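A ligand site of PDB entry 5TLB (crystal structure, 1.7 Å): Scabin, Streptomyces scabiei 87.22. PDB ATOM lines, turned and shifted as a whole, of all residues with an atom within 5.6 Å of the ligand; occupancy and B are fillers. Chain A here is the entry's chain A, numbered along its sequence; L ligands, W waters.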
ATOM      1  N   TYR A  76       1.865  20.029  13.552  1.00  0.00           N
ATOM      2  CA  TYR A  76       0.662  20.605  12.973  1.00  0.00           C
ATOM      3  C   TYR A  76      -0.429  20.696  14.024  1.00  0.00           C
ATOM      4  O   TYR A  76      -0.455  19.942  15.001  1.00  0.00           O
ATOM      5  CB  TYR A  76       0.171  19.775  11.777  1.00  0.00           C
ATOM      6  CG  TYR A  76       1.302  19.490  10.825  1.00  0.00           C
ATOM      7  CD1 TYR A  76       2.123  18.394  11.029  1.00  0.00           C
ATOM      8  CD2 TYR A  76       1.578  20.339   9.759  1.00  0.00           C
ATOM      9  CE1 TYR A  76       3.182  18.131  10.184  1.00  0.00           C
ATOM     10  CE2 TYR A  76       2.651  20.078   8.910  1.00  0.00           C
ATOM     11  CZ  TYR A  76       3.442  18.971   9.134  1.00  0.00           C
ATOM     12  OH  TYR A  76       4.515  18.672   8.323  1.00  0.00           O
ATOM     13  N   ARG A  77      -1.348  21.634  13.809  1.00  0.00           N
ATOM     14  CA  ARG A  77      -2.495  21.765  14.693  1.00  0.00           C
ATOM     15  C   ARG A  77      -3.697  22.243  13.891  1.00  0.00           C
ATOM     16  O   ARG A  77      -3.617  23.264  13.191  1.00  0.00           O
ATOM     17  CB  ARG A  77      -2.199  22.723  15.838  1.00  0.00           C
ATOM     18  CG  ARG A  77      -3.443  22.994  16.688  1.00  0.00           C
ATOM     19  CD  ARG A  77      -3.165  23.844  17.903  1.00  0.00           C
ATOM     20  NE  ARG A  77      -4.442  24.300  18.447  1.00  0.00           N
ATOM     21  CZ  ARG A  77      -5.234  23.562  19.210  1.00  0.00           C
ATOM     22  NH1 ARG A  77      -6.395  24.069  19.631  1.00  0.00           N
ATOM     23  NH2 ARG A  77      -4.891  22.327  19.567  1.00  0.00           N
ATOM     24  N   SER A  78      -4.806  21.511  14.007  1.00  0.00           N
ATOM     25  CA  SER A  78      -6.079  21.971  13.488  1.00  0.00           C
ATOM     26  C   SER A  78      -6.705  22.940  14.475  1.00  0.00           C
ATOM     27  O   SER A  78      -6.837  22.628  15.662  1.00  0.00           O
ATOM     28  CB  SER A  78      -7.011  20.783  13.258  1.00  0.00           C
ATOM     29  OG  SER A  78      -6.626  20.046  12.132  1.00  0.00           O
ATOM     30  N   ASP A  79      -7.101  24.106  13.985  1.00  0.00           N
ATOM     31  CA  ASP A  79      -7.680  25.125  14.838  1.00  0.00           C
ATOM     32  C   ASP A  79      -8.630  25.943  13.977  1.00  0.00           C
ATOM     33  O   ASP A  79      -8.296  26.277  12.839  1.00  0.00           O
ATOM     34  CB  ASP A  79      -6.584  25.989  15.484  1.00  0.00           C
ATOM     35  CG  ASP A  79      -7.045  26.681  16.747  1.00  0.00           C
ATOM     36  OD1 ASP A  79      -7.984  27.497  16.667  1.00  0.00           O
ATOM     37  OD2 ASP A  79      -6.455  26.420  17.818  1.00  0.00           O
ATOM     38  N   SER A  80      -9.817  26.207  14.503  1.00  0.00           N
ATOM     39  CA  SER A  80     -10.791  26.995  13.760  1.00  0.00           C
ATOM     40  C   SER A  80     -10.504  28.493  13.815  1.00  0.00           C
ATOM     41  O   SER A  80     -11.131  29.258  13.063  1.00  0.00           O
ATOM     42  CB  SER A  80     -12.198  26.738  14.307  1.00  0.00           C
ATOM     43  OG  SER A  80     -12.273  27.107  15.676  1.00  0.00           O
ATOM     44  N   ARG A  81      -9.607  28.940  14.682  1.00  0.00           N
ATOM     45  CA  ARG A  81      -9.294  30.357  14.792  1.00  0.00           C
ATOM     46  C   ARG A  81      -8.387  30.803  13.653  1.00  0.00           C
ATOM     47  O   ARG A  81      -7.474  30.078  13.257  1.00  0.00           O
ATOM     48  CB  ARG A  81      -8.633  30.639  16.133  1.00  0.00           C
ATOM     49  CG  ARG A  81      -9.594  30.575  17.310  1.00  0.00           C
ATOM     50  CD  ARG A  81      -8.853  30.717  18.624  1.00  0.00           C
ATOM     51  NE  ARG A  81      -7.916  29.626  18.797  1.00  0.00           N
ATOM     52  CZ  ARG A  81      -6.961  29.588  19.722  1.00  0.00           C
ATOM     53  NH1 ARG A  81      -6.810  30.601  20.570  1.00  0.00           N
ATOM     54  NH2 ARG A  81      -6.150  28.527  19.795  1.00  0.00           N
ATOM     55  N   LEU A  92      -2.486  29.709  23.180  1.00  0.00           N
ATOM     56  CA  LEU A  92      -2.642  29.713  24.624  1.00  0.00           C
ATOM     57  C   LEU A  92      -3.468  28.515  25.081  1.00  0.00           C
ATOM     58  O   LEU A  92      -4.448  28.148  24.422  1.00  0.00           O
ATOM     59  CB  LEU A  92      -3.311  31.010  25.090  1.00  0.00           C
ATOM     60  CG  LEU A  92      -2.402  32.239  25.114  1.00  0.00           C
ATOM     61  CD1 LEU A  92      -3.200  33.524  25.275  1.00  0.00           C
ATOM     62  CD2 LEU A  92      -1.391  32.123  26.242  1.00  0.00           C
ATOM     63  N   PRO A  93      -3.099  27.879  26.192  1.00  0.00           N
ATOM     64  CA  PRO A  93      -3.919  26.793  26.734  1.00  0.00           C
ATOM     65  C   PRO A  93      -5.149  27.336  27.450  1.00  0.00           C
ATOM     66  O   PRO A  93      -5.187  28.468  27.925  1.00  0.00           O
ATOM     67  CB  PRO A  93      -2.973  26.100  27.708  1.00  0.00           C
ATOM     68  CG  PRO A  93      -2.121  27.235  28.225  1.00  0.00           C
ATOM     69  CD  PRO A  93      -1.936  28.168  27.057  1.00  0.00           C
ATOM     70  N   LYS A  94      -6.158  26.469  27.564  1.00  0.00           N
ATOM     71  CA  LYS A  94      -7.447  26.907  28.079  1.00  0.00           C
ATOM     72  C   LYS A  94      -7.444  27.104  29.593  1.00  0.00           C
ATOM     73  O   LYS A  94      -8.161  27.977  30.086  1.00  0.00           O
ATOM     74  CB  LYS A  94      -8.535  25.909  27.668  1.00  0.00           C
ATOM     75  CG  LYS A  94      -8.890  26.043  26.208  1.00  0.00           C
ATOM     76  CD  LYS A  94     -10.109  25.229  25.826  1.00  0.00           C
ATOM     77  CE  LYS A  94     -10.560  25.618  24.425  1.00  0.00           C
ATOM     78  NZ  LYS A  94     -11.585  24.694  23.873  1.00  0.00           N
ATOM     79  N   TYR A 106      -7.153  13.865  29.407  1.00  0.00           N
ATOM     80  CA  TYR A 106      -7.301  14.922  28.419  1.00  0.00           C
ATOM     81  C   TYR A 106      -7.451  14.356  27.010  1.00  0.00           C
ATOM     82  O   TYR A 106      -8.268  14.841  26.216  1.00  0.00           O
ATOM     83  CB  TYR A 106      -6.114  15.880  28.508  1.00  0.00           C
ATOM     84  CG  TYR A 106      -6.011  16.825  27.340  1.00  0.00           C
ATOM     85  CD1 TYR A 106      -6.933  17.834  27.152  1.00  0.00           C
ATOM     86  CD2 TYR A 106      -4.987  16.708  26.413  1.00  0.00           C
ATOM     87  CE1 TYR A 106      -6.851  18.695  26.083  1.00  0.00           C
ATOM     88  CE2 TYR A 106      -4.890  17.563  25.344  1.00  0.00           C
ATOM     89  CZ  TYR A 106      -5.832  18.557  25.185  1.00  0.00           C
ATOM     90  OH  TYR A 106      -5.748  19.409  24.119  1.00  0.00           O
ATOM     91  N   VAL A 107      -6.669  13.325  26.673  1.00  0.00           N
ATOM     92  CA  VAL A 107      -6.777  12.719  25.343  1.00  0.00           C
ATOM     93  C   VAL A 107      -8.141  12.064  25.178  1.00  0.00           C
ATOM     94  O   VAL A 107      -8.784  12.187  24.135  1.00  0.00           O
ATOM     95  CB  VAL A 107      -5.640  11.699  25.132  1.00  0.00           C
ATOM     96  CG1 VAL A 107      -5.910  10.838  23.888  1.00  0.00           C
ATOM     97  CG2 VAL A 107      -4.304  12.420  25.005  1.00  0.00           C
ATOM     98  N   LEU A 108      -8.593  11.343  26.205  1.00  0.00           N
ATOM     99  CA  LEU A 108      -9.820  10.570  26.071  1.00  0.00           C
ATOM    100  C   LEU A 108     -11.049  11.469  26.113  1.00  0.00           C
ATOM    101  O   LEU A 108     -11.985  11.313  25.322  1.00  0.00           O
ATOM    102  CB  LEU A 108      -9.894   9.521  27.176  1.00  0.00           C
ATOM    103  CG  LEU A 108     -10.968   8.447  27.000  1.00  0.00           C
ATOM    104  CD1 LEU A 108     -10.605   7.535  25.834  1.00  0.00           C
ATOM    105  N   VAL A 109     -11.058  12.395  27.061  1.00  0.00           N
ATOM    106  CA  VAL A 109     -12.149  13.341  27.239  1.00  0.00           C
ATOM    107  C   VAL A 109     -11.519  14.711  27.123  1.00  0.00           C
ATOM    108  O   VAL A 109     -10.897  15.212  28.067  1.00  0.00           O
ATOM    109  CB  VAL A 109     -12.833  13.168  28.597  1.00  0.00           C
ATOM    110  CG1 VAL A 109     -13.946  14.193  28.760  1.00  0.00           C
ATOM    111  CG2 VAL A 109     -13.363  11.756  28.734  1.00  0.00           C
ATOM    112  N   ASN A 110     -11.627  15.315  25.941  1.00  0.00           N
ATOM    113  CA  ASN A 110     -11.177  16.684  25.785  1.00  0.00           C
ATOM    114  C   ASN A 110     -11.925  17.559  26.787  1.00  0.00           C
ATOM    115  O   ASN A 110     -13.155  17.506  26.882  1.00  0.00           O
ATOM    116  CB  ASN A 110     -11.434  17.145  24.350  1.00  0.00           C
ATOM    117  CG  ASN A 110     -10.690  18.415  23.990  1.00  0.00           C
ATOM    118  OD1 ASN A 110      -9.706  18.788  24.637  1.00  0.00           O
ATOM    119  ND2 ASN A 110     -11.155  19.083  22.952  1.00  0.00           N
ATOM    120  N   TYR A 115      -2.676  22.108  28.277  1.00  0.00           N
ATOM    121  CA  TYR A 115      -2.009  21.659  27.065  1.00  0.00           C
ATOM    122  C   TYR A 115      -2.615  22.265  25.818  1.00  0.00           C
ATOM    123  O   TYR A 115      -3.829  22.483  25.729  1.00  0.00           O
ATOM    124  CB  TYR A 115      -2.087  20.128  26.942  1.00  0.00           C
ATOM    125  CG  TYR A 115      -1.596  19.394  28.158  1.00  0.00           C
ATOM    126  CD1 TYR A 115      -0.240  19.376  28.479  1.00  0.00           C
ATOM    127  CD2 TYR A 115      -2.470  18.690  28.967  1.00  0.00           C
ATOM    128  CE1 TYR A 115       0.221  18.694  29.607  1.00  0.00           C
ATOM    129  CE2 TYR A 115      -2.019  17.996  30.078  1.00  0.00           C
ATOM    130  CZ  TYR A 115      -0.674  18.013  30.406  1.00  0.00           C
ATOM    131  OH  TYR A 115      -0.233  17.324  31.508  1.00  0.00           O
ATOM    132  N   VAL A 116      -1.759  22.518  24.826  1.00  0.00           N
ATOM    133  CA  VAL A 116      -2.184  22.734  23.456  1.00  0.00           C
ATOM    134  C   VAL A 116      -1.764  21.520  22.648  1.00  0.00           C
ATOM    135  O   VAL A 116      -0.587  21.142  22.643  1.00  0.00           O
ATOM    136  CB  VAL A 116      -1.606  24.029  22.869  1.00  0.00           C
ATOM    137  CG1 VAL A 116      -1.918  24.114  21.379  1.00  0.00           C
ATOM    138  CG2 VAL A 116      -2.168  25.226  23.606  1.00  0.00           C
ATOM    139  N   SER A 117      -2.727  20.908  21.972  1.00  0.00           N
ATOM    140  CA  SER A 117      -2.494  19.688  21.209  1.00  0.00           C
ATOM    141  C   SER A 117      -1.962  20.002  19.826  1.00  0.00           C
ATOM    142  O   SER A 117      -2.422  20.934  19.157  1.00  0.00           O
ATOM    143  CB  SER A 117      -3.785  18.880  21.089  1.00  0.00           C
ATOM    144  OG  SER A 117      -4.120  18.285  22.328  1.00  0.00           O
ATOM    145  N   THR A 118      -0.988  19.197  19.396  1.00  0.00           N
ATOM    146  CA  THR A 118      -0.418  19.219  18.052  1.00  0.00           C
ATOM    147  C   THR A 118      -0.215  17.772  17.638  1.00  0.00           C
ATOM    148  O   THR A 118      -0.361  16.847  18.452  1.00  0.00           O
ATOM    149  CB  THR A 118       0.914  19.980  17.986  1.00  0.00           C
ATOM    150  OG1 THR A 118       1.912  19.213  18.664  1.00  0.00           O
ATOM    151  CG2 THR A 118       0.783  21.358  18.637  1.00  0.00           C
ATOM    152  N   THR A 119       0.138  17.570  16.380  1.00  0.00           N
ATOM    153  CA  THR A 119       0.330  16.235  15.850  1.00  0.00           C
ATOM    154  C   THR A 119       1.581  16.199  14.961  1.00  0.00           C
ATOM    155  O   THR A 119       1.937  17.180  14.306  1.00  0.00           O
ATOM    156  CB  THR A 119      -0.894  15.778  15.054  1.00  0.00           C
ATOM    157  OG1 THR A 119      -0.671  14.469  14.512  1.00  0.00           O
ATOM    158  CG2 THR A 119      -1.221  16.750  13.924  1.00  0.00           C
ATOM    159  N   LEU A 124      -3.579  15.042   9.556  1.00  0.00           N
ATOM    160  CA  LEU A 124      -4.612  14.802  10.556  1.00  0.00           C
ATOM    161  C   LEU A 124      -5.771  15.771  10.400  1.00  0.00           C
ATOM    162  O   LEU A 124      -6.889  15.456  10.829  1.00  0.00           O
ATOM    163  CB  LEU A 124      -4.033  14.912  11.966  1.00  0.00           C
ATOM    164  CG  LEU A 124      -4.976  14.311  13.023  1.00  0.00           C
ATOM    165  CD1 LEU A 124      -5.029  12.809  12.897  1.00  0.00           C
ATOM    166  CD2 LEU A 124      -4.565  14.706  14.430  1.00  0.00           C
ATOM    167  N   TRP A 128     -10.734  16.254  10.946  1.00  0.00           N
ATOM    168  CA  TRP A 128     -11.507  17.233  11.685  1.00  0.00           C
ATOM    169  C   TRP A 128     -12.778  17.609  10.926  1.00  0.00           C
ATOM    170  O   TRP A 128     -12.810  17.644   9.690  1.00  0.00           O
ATOM    171  CB  TRP A 128     -10.679  18.479  11.975  1.00  0.00           C
ATOM    172  CG  TRP A 128     -10.307  18.529  13.404  1.00  0.00           C
ATOM    173  CD1 TRP A 128     -10.873  19.298  14.392  1.00  0.00           C
ATOM    174  CD2 TRP A 128      -9.320  17.729  14.046  1.00  0.00           C
ATOM    175  NE1 TRP A 128     -10.275  19.025  15.598  1.00  0.00           N
ATOM    176  CE2 TRP A 128      -9.313  18.070  15.407  1.00  0.00           C
ATOM    177  CE3 TRP A 128      -8.418  16.763  13.586  1.00  0.00           C
ATOM    178  CZ2 TRP A 128      -8.448  17.473  16.318  1.00  0.00           C
ATOM    179  CZ3 TRP A 128      -7.565  16.185  14.497  1.00  0.00           C
ATOM    180  CH2 TRP A 128      -7.591  16.534  15.844  1.00  0.00           C
ATOM    181  N   SER A 131     -12.567  22.160  10.784  1.00  0.00           N
ATOM    182  CA  SER A 131     -11.574  22.804  11.624  1.00  0.00           C
ATOM    183  C   SER A 131     -10.924  24.008  10.976  1.00  0.00           C
ATOM    184  O   SER A 131     -10.134  24.685  11.647  1.00  0.00           O
ATOM    185  CB  SER A 131     -10.465  21.847  12.020  1.00  0.00           C
ATOM    186  OG  SER A 131      -9.422  22.610  12.607  1.00  0.00           O
ATOM    187  N   GLN A 158      -3.696   9.646  16.447  1.00  0.00           N
ATOM    188  CA  GLN A 158      -3.503  11.076  16.303  1.00  0.00           C
ATOM    189  C   GLN A 158      -2.053  11.487  16.439  1.00  0.00           C
ATOM    190  O   GLN A 158      -1.742  12.662  16.176  1.00  0.00           O
ATOM    191  CB  GLN A 158      -4.320  11.834  17.341  1.00  0.00           C
ATOM    192  CG  GLN A 158      -5.822  11.690  17.216  1.00  0.00           C
ATOM    193  CD  GLN A 158      -6.566  12.502  18.253  1.00  0.00           C
ATOM    194  OE1 GLN A 158      -6.230  12.470  19.440  1.00  0.00           O
ATOM    195  NE2 GLN A 158      -7.554  13.264  17.812  1.00  0.00           N
ATOM    196  N   VAL A 159      -1.180  10.567  16.856  1.00  0.00           N
ATOM    197  CA  VAL A 159       0.252  10.809  17.054  1.00  0.00           C
ATOM    198  C   VAL A 159       0.491  12.216  17.583  1.00  0.00           C
ATOM    199  O   VAL A 159       1.145  13.058  16.942  1.00  0.00           O
ATOM    200  CB  VAL A 159       1.037  10.511  15.756  1.00  0.00           C
ATOM    201  CG1 VAL A 159       0.992   9.013  15.495  1.00  0.00           C
ATOM    202  CG2 VAL A 159       0.473  11.268  14.557  1.00  0.00           C
ATOM    203  N   GLU A 160      -0.028  12.450  18.787  1.00  0.00           N
ATOM    204  CA  GLU A 160      -0.116  13.772  19.372  1.00  0.00           C
ATOM    205  C   GLU A 160       1.150  14.172  20.125  1.00  0.00           C
ATOM    206  O   GLU A 160       1.845  13.326  20.697  1.00  0.00           O
ATOM    207  CB  GLU A 160      -1.313  13.823  20.332  1.00  0.00           C
ATOM    208  CG  GLU A 160      -1.584  15.183  20.888  1.00  0.00           C
ATOM    209  CD  GLU A 160      -2.729  15.198  21.860  1.00  0.00           C
ATOM    210  OE1 GLU A 160      -3.503  14.219  21.871  1.00  0.00           O
ATOM    211  OE2 GLU A 160      -2.851  16.188  22.606  1.00  0.00           O
ATOM    212  N   VAL A 161       1.425  15.468  20.104  1.00  0.00           N
ATOM    213  CA  VAL A 161       2.409  16.108  20.964  1.00  0.00           C
ATOM    214  C   VAL A 161       1.670  17.211  21.703  1.00  0.00           C
ATOM    215  O   VAL A 161       1.126  18.125  21.067  1.00  0.00           O
ATOM    216  CB  VAL A 161       3.602  16.679  20.171  1.00  0.00           C
ATOM    217  CG1 VAL A 161       4.589  17.348  21.113  1.00  0.00           C
ATOM    218  CG2 VAL A 161       4.304  15.569  19.370  1.00  0.00           C
HETATM  219  P1  LIG L   1      -8.854  22.587  21.848  1.00  0.00           P
HETATM  220  O1  LIG L   1      -9.888  22.846  22.903  1.00  0.00           O
HETATM  221  O2  LIG L   1      -7.392  22.902  21.944  1.00  0.00           O
HETATM  222  O3  LIG L   1      -9.359  23.657  20.574  1.00  0.00           O
HETATM  223  C1  LIG L   1     -10.716  23.484  20.309  1.00  0.00           C
HETATM  224  C2  LIG L   1     -11.200  24.802  19.736  1.00  0.00           C
HETATM  225  O4  LIG L   1     -11.298  25.711  20.815  1.00  0.00           O
HETATM  226  C3  LIG L   1     -10.127  25.408  18.757  1.00  0.00           C
HETATM  227  O5  LIG L   1     -10.390  24.943  17.452  1.00  0.00           O
HETATM  228  C4  LIG L   1     -10.428  26.890  18.902  1.00  0.00           C
HETATM  229  O6  LIG L   1     -11.567  27.288  18.181  1.00  0.00           O
HETATM  230  C5  LIG L   1     -10.799  26.991  20.429  1.00  0.00           C
HETATM  231  N1  LIG L   1      -9.652  27.287  21.317  1.00  0.00           N
HETATM  232  C6  LIG L   1      -8.523  26.506  21.637  1.00  0.00           C
HETATM  233  N2  LIG L   1      -7.711  27.126  22.531  1.00  0.00           N
HETATM  234  C7  LIG L   1      -8.359  28.347  22.807  1.00  0.00           C
HETATM  235  C8  LIG L   1      -8.020  29.434  23.654  1.00  0.00           C
HETATM  236  N3  LIG L   1      -6.886  29.430  24.406  1.00  0.00           N
HETATM  237  N4  LIG L   1      -8.838  30.528  23.743  1.00  0.00           N
HETATM  238  C9  LIG L   1      -9.968  30.477  22.972  1.00  0.00           C
HETATM  239  N5  LIG L   1     -10.424  29.531  22.126  1.00  0.00           N
HETATM  240  C10 LIG L   1      -9.562  28.457  22.075  1.00  0.00           C
HETATM  241  O7  LIG L   1      -9.254  21.078  21.436  1.00  0.00           O
HETATM  242  P2  LIG L   1      -8.544  20.566  20.072  1.00  0.00           P
HETATM  243  O8  LIG L   1      -7.091  20.840  19.883  1.00  0.00           O
HETATM  244  O9  LIG L   1      -9.670  20.829  19.096  1.00  0.00           O
HETATM  245  O10 LIG L   1      -8.648  18.854  20.085  1.00  0.00           O
HETATM  246  C11 LIG L   1      -8.164  18.399  21.289  1.00  0.00           C
HETATM  247  C12 LIG L   1      -8.441  16.920  21.311  1.00  0.00           C
HETATM  248  O11 LIG L   1      -7.926  16.389  20.065  1.00  0.00           O
HETATM  249  C13 LIG L   1      -7.653  16.291  22.482  1.00  0.00           C
HETATM  250  O12 LIG L   1      -8.367  15.178  22.930  1.00  0.00           O
HETATM  251  C14 LIG L   1      -6.319  15.913  21.829  1.00  0.00           C
HETATM  252  O13 LIG L   1      -5.850  14.694  22.286  1.00  0.00           O
HETATM  253  C15 LIG L   1      -6.706  15.723  20.290  1.00  0.00           C
HETATM  254  N6  LIG L   1      -5.655  16.285  19.373  1.00  0.00           N
HETATM  255  C16 LIG L   1      -5.836  17.507  18.692  1.00  0.00           C
HETATM  256  C17 LIG L   1      -4.928  17.868  17.705  1.00  0.00           C
HETATM  257  C18 LIG L   1      -5.226  18.980  16.795  1.00  0.00           C
HETATM  258  O14 LIG L   1      -4.667  19.105  15.666  1.00  0.00           O
HETATM  259  N7  LIG L   1      -6.142  19.952  17.205  1.00  0.00           N
HETATM  260  C19 LIG L   1      -3.642  17.146  17.500  1.00  0.00           C
HETATM  261  C20 LIG L   1      -3.650  15.812  18.154  1.00  0.00           C
HETATM  262  C21 LIG L   1      -4.476  15.546  19.172  1.00  0.00           C
HETATM  263  O   HOH W   1      -4.502  27.333  21.990  1.00  0.00           O
HETATM  264  O   HOH W   2     -13.231  24.490  16.546  1.00  0.00           O
HETATM  265  O   HOH W   3      -4.747  18.203  12.886  1.00  0.00           O
HETATM  266  O   HOH W   4      -6.023  24.997  23.069  1.00  0.00           O
HETATM  267  O   HOH W   5      -5.444  21.643  22.842  1.00  0.00           O
HETATM  268  O   HOH W   6      -6.787  31.386  26.331  1.00  0.00           O
HETATM  269  O   HOH W   7      -9.460  32.720  25.156  1.00  0.00           O
HETATM  270  O   HOH W   8      -8.258  32.922  21.148  1.00  0.00           O
HETATM  271  O   HOH W   9      -9.187  22.647  17.108  1.00  0.00           O
HETATM  272  O   HOH W  10      -9.302  21.428  25.427  1.00  0.00           O
HETATM  273  O   HOH W  11     -11.983  20.011  19.247  1.00  0.00           O
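The side-chain carboxylate (OE1) of Glu 160 sits at hydrogen-bond distance from an oxygen (O13) of the ligand (2.4 Å).
An oxygen (O5) of the ligand lies within hydrogen-bond range of the backbone NH of Ser 80 (3.3 Å).
The side-chain hydroxyl of Ser 80 lies within hydrogen-bond range of an oxygen (O6) of the ligand (2.6 Å).
An oxygen (O8) of the ligand is in salt-bridge range of the guanidinium group (NH2) of Arg 77, at 2.7 Å.
An oxygen (O1) of the ligand is in salt-bridge range of the side-chain amino group of Lys 94 (2.7 Å).
The backbone carbonyl oxygen of Leu 92 lies within hydrogen-bond range of a nitrogen (N3) of the ligand (2.8 Å).
O14 of the ligand lies within hydrogen-bond range of N of Ser 78.
The backbone carbonyl oxygen (O) of Ser 78 sits at hydrogen-bond distance from a nitrogen (N7) of the ligand.
The side-chain amide nitrogen (ND2) of Asn 110 lies within hydrogen-bond range of an oxygen (O7) of the ligand.
O of Val 107 sits at hydrogen-bond distance from O12 of the ligand (3.3 Å).
The backbone carbonyl oxygen (O) of Tyr 106 lies within hydrogen-bond range of an oxygen (O12) of the ligand.
The guanidinium group of Arg 81 lies within hydrogen-bond range of a nitrogen (N2) of the ligand, at 3.4 Å.
OG of Ser 117 sits at hydrogen-bond distance from OE2 of Glu 160 (2.5 Å).
NH2 of Arg 77 sits at hydrogen-bond distance from O of Ser 117 (2.9 Å).
OD2 of Asp 79 lies within salt-bridge range of NH1 of Arg 77.
The side-chain hydroxyl (OH) of Tyr 106 is in hydrogen-bond range of the side-chain hydroxyl (OG) of Ser 117 (2.7 Å).
The guanidinium group (NH2) of Arg 81 lies within salt-bridge range of the side-chain carboxylate (OD2) of Asp 79 (2.9 Å).
The backbone NH (N) of Asp 79 sits at hydrogen-bond distance from the side-chain hydroxyl (OG) of Ser 131 (3.1 Å).
The backbone carbonyl oxygen (O) of Tyr 76 lies within hydrogen-bond range of the backbone NH (N) of Thr 119 (2.8 Å).
The side-chain hydroxyl of Thr 119 sits at hydrogen-bond distance from the backbone carbonyl oxygen of Val 159 (3.3 Å).
Residues that only touch the ligand: Ser 117, Asp 79, Gln 158, Thr 118, Trp 128, Thr 119 and Leu 124.
Hydrophobic or aromatic side chains within 4 Å of the ligand: Leu 92, Tyr 106, Val 107, Leu 124 and Trp 128.
17 residues have an atom within 4 Å of the ligand: Arg 77, Ser 78, Asp 79, Ser 80, Arg 81, Leu 92, Lys 94, Tyr 106, Val 107, Asn 110, Ser 117, Thr 118, Thr 119, Leu 124, Trp 128, Gln 158 and Glu 160.
The nearest printed residue that does not touch the ligand is Pro 93 (4.02 Å).
Water W5 lies within hydrogen-bond range of O2 of the ligand, OH of Tyr 106, N of Ser 117, NH2 of Arg 77 and O of Tyr 115.
Water W9 bridges an oxygen (O5) of the ligand and the backbone carbonyl oxygen (O) of Ser 78.
Water W3 lies within hydrogen-bond range of OG of Ser 78 (2.7 Å) and O14 of the ligand (2.9 Å).
Water W10 bridges the side-chain amide oxygen of Asn 110 and an oxygen (O1) of the ligand.
Water W2 bridges the side-chain hydroxyl (OG) of Ser 80 (2.9 Å) and an oxygen (O5) of the ligand (3.0 Å).
Water W1 lies within hydrogen-bond range of the backbone carbonyl oxygen of Leu 92 (2.6 Å), the guanidinium group of Arg 81 (3.0 Å) and a nitrogen (N2) of the ligand (3.3 Å).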
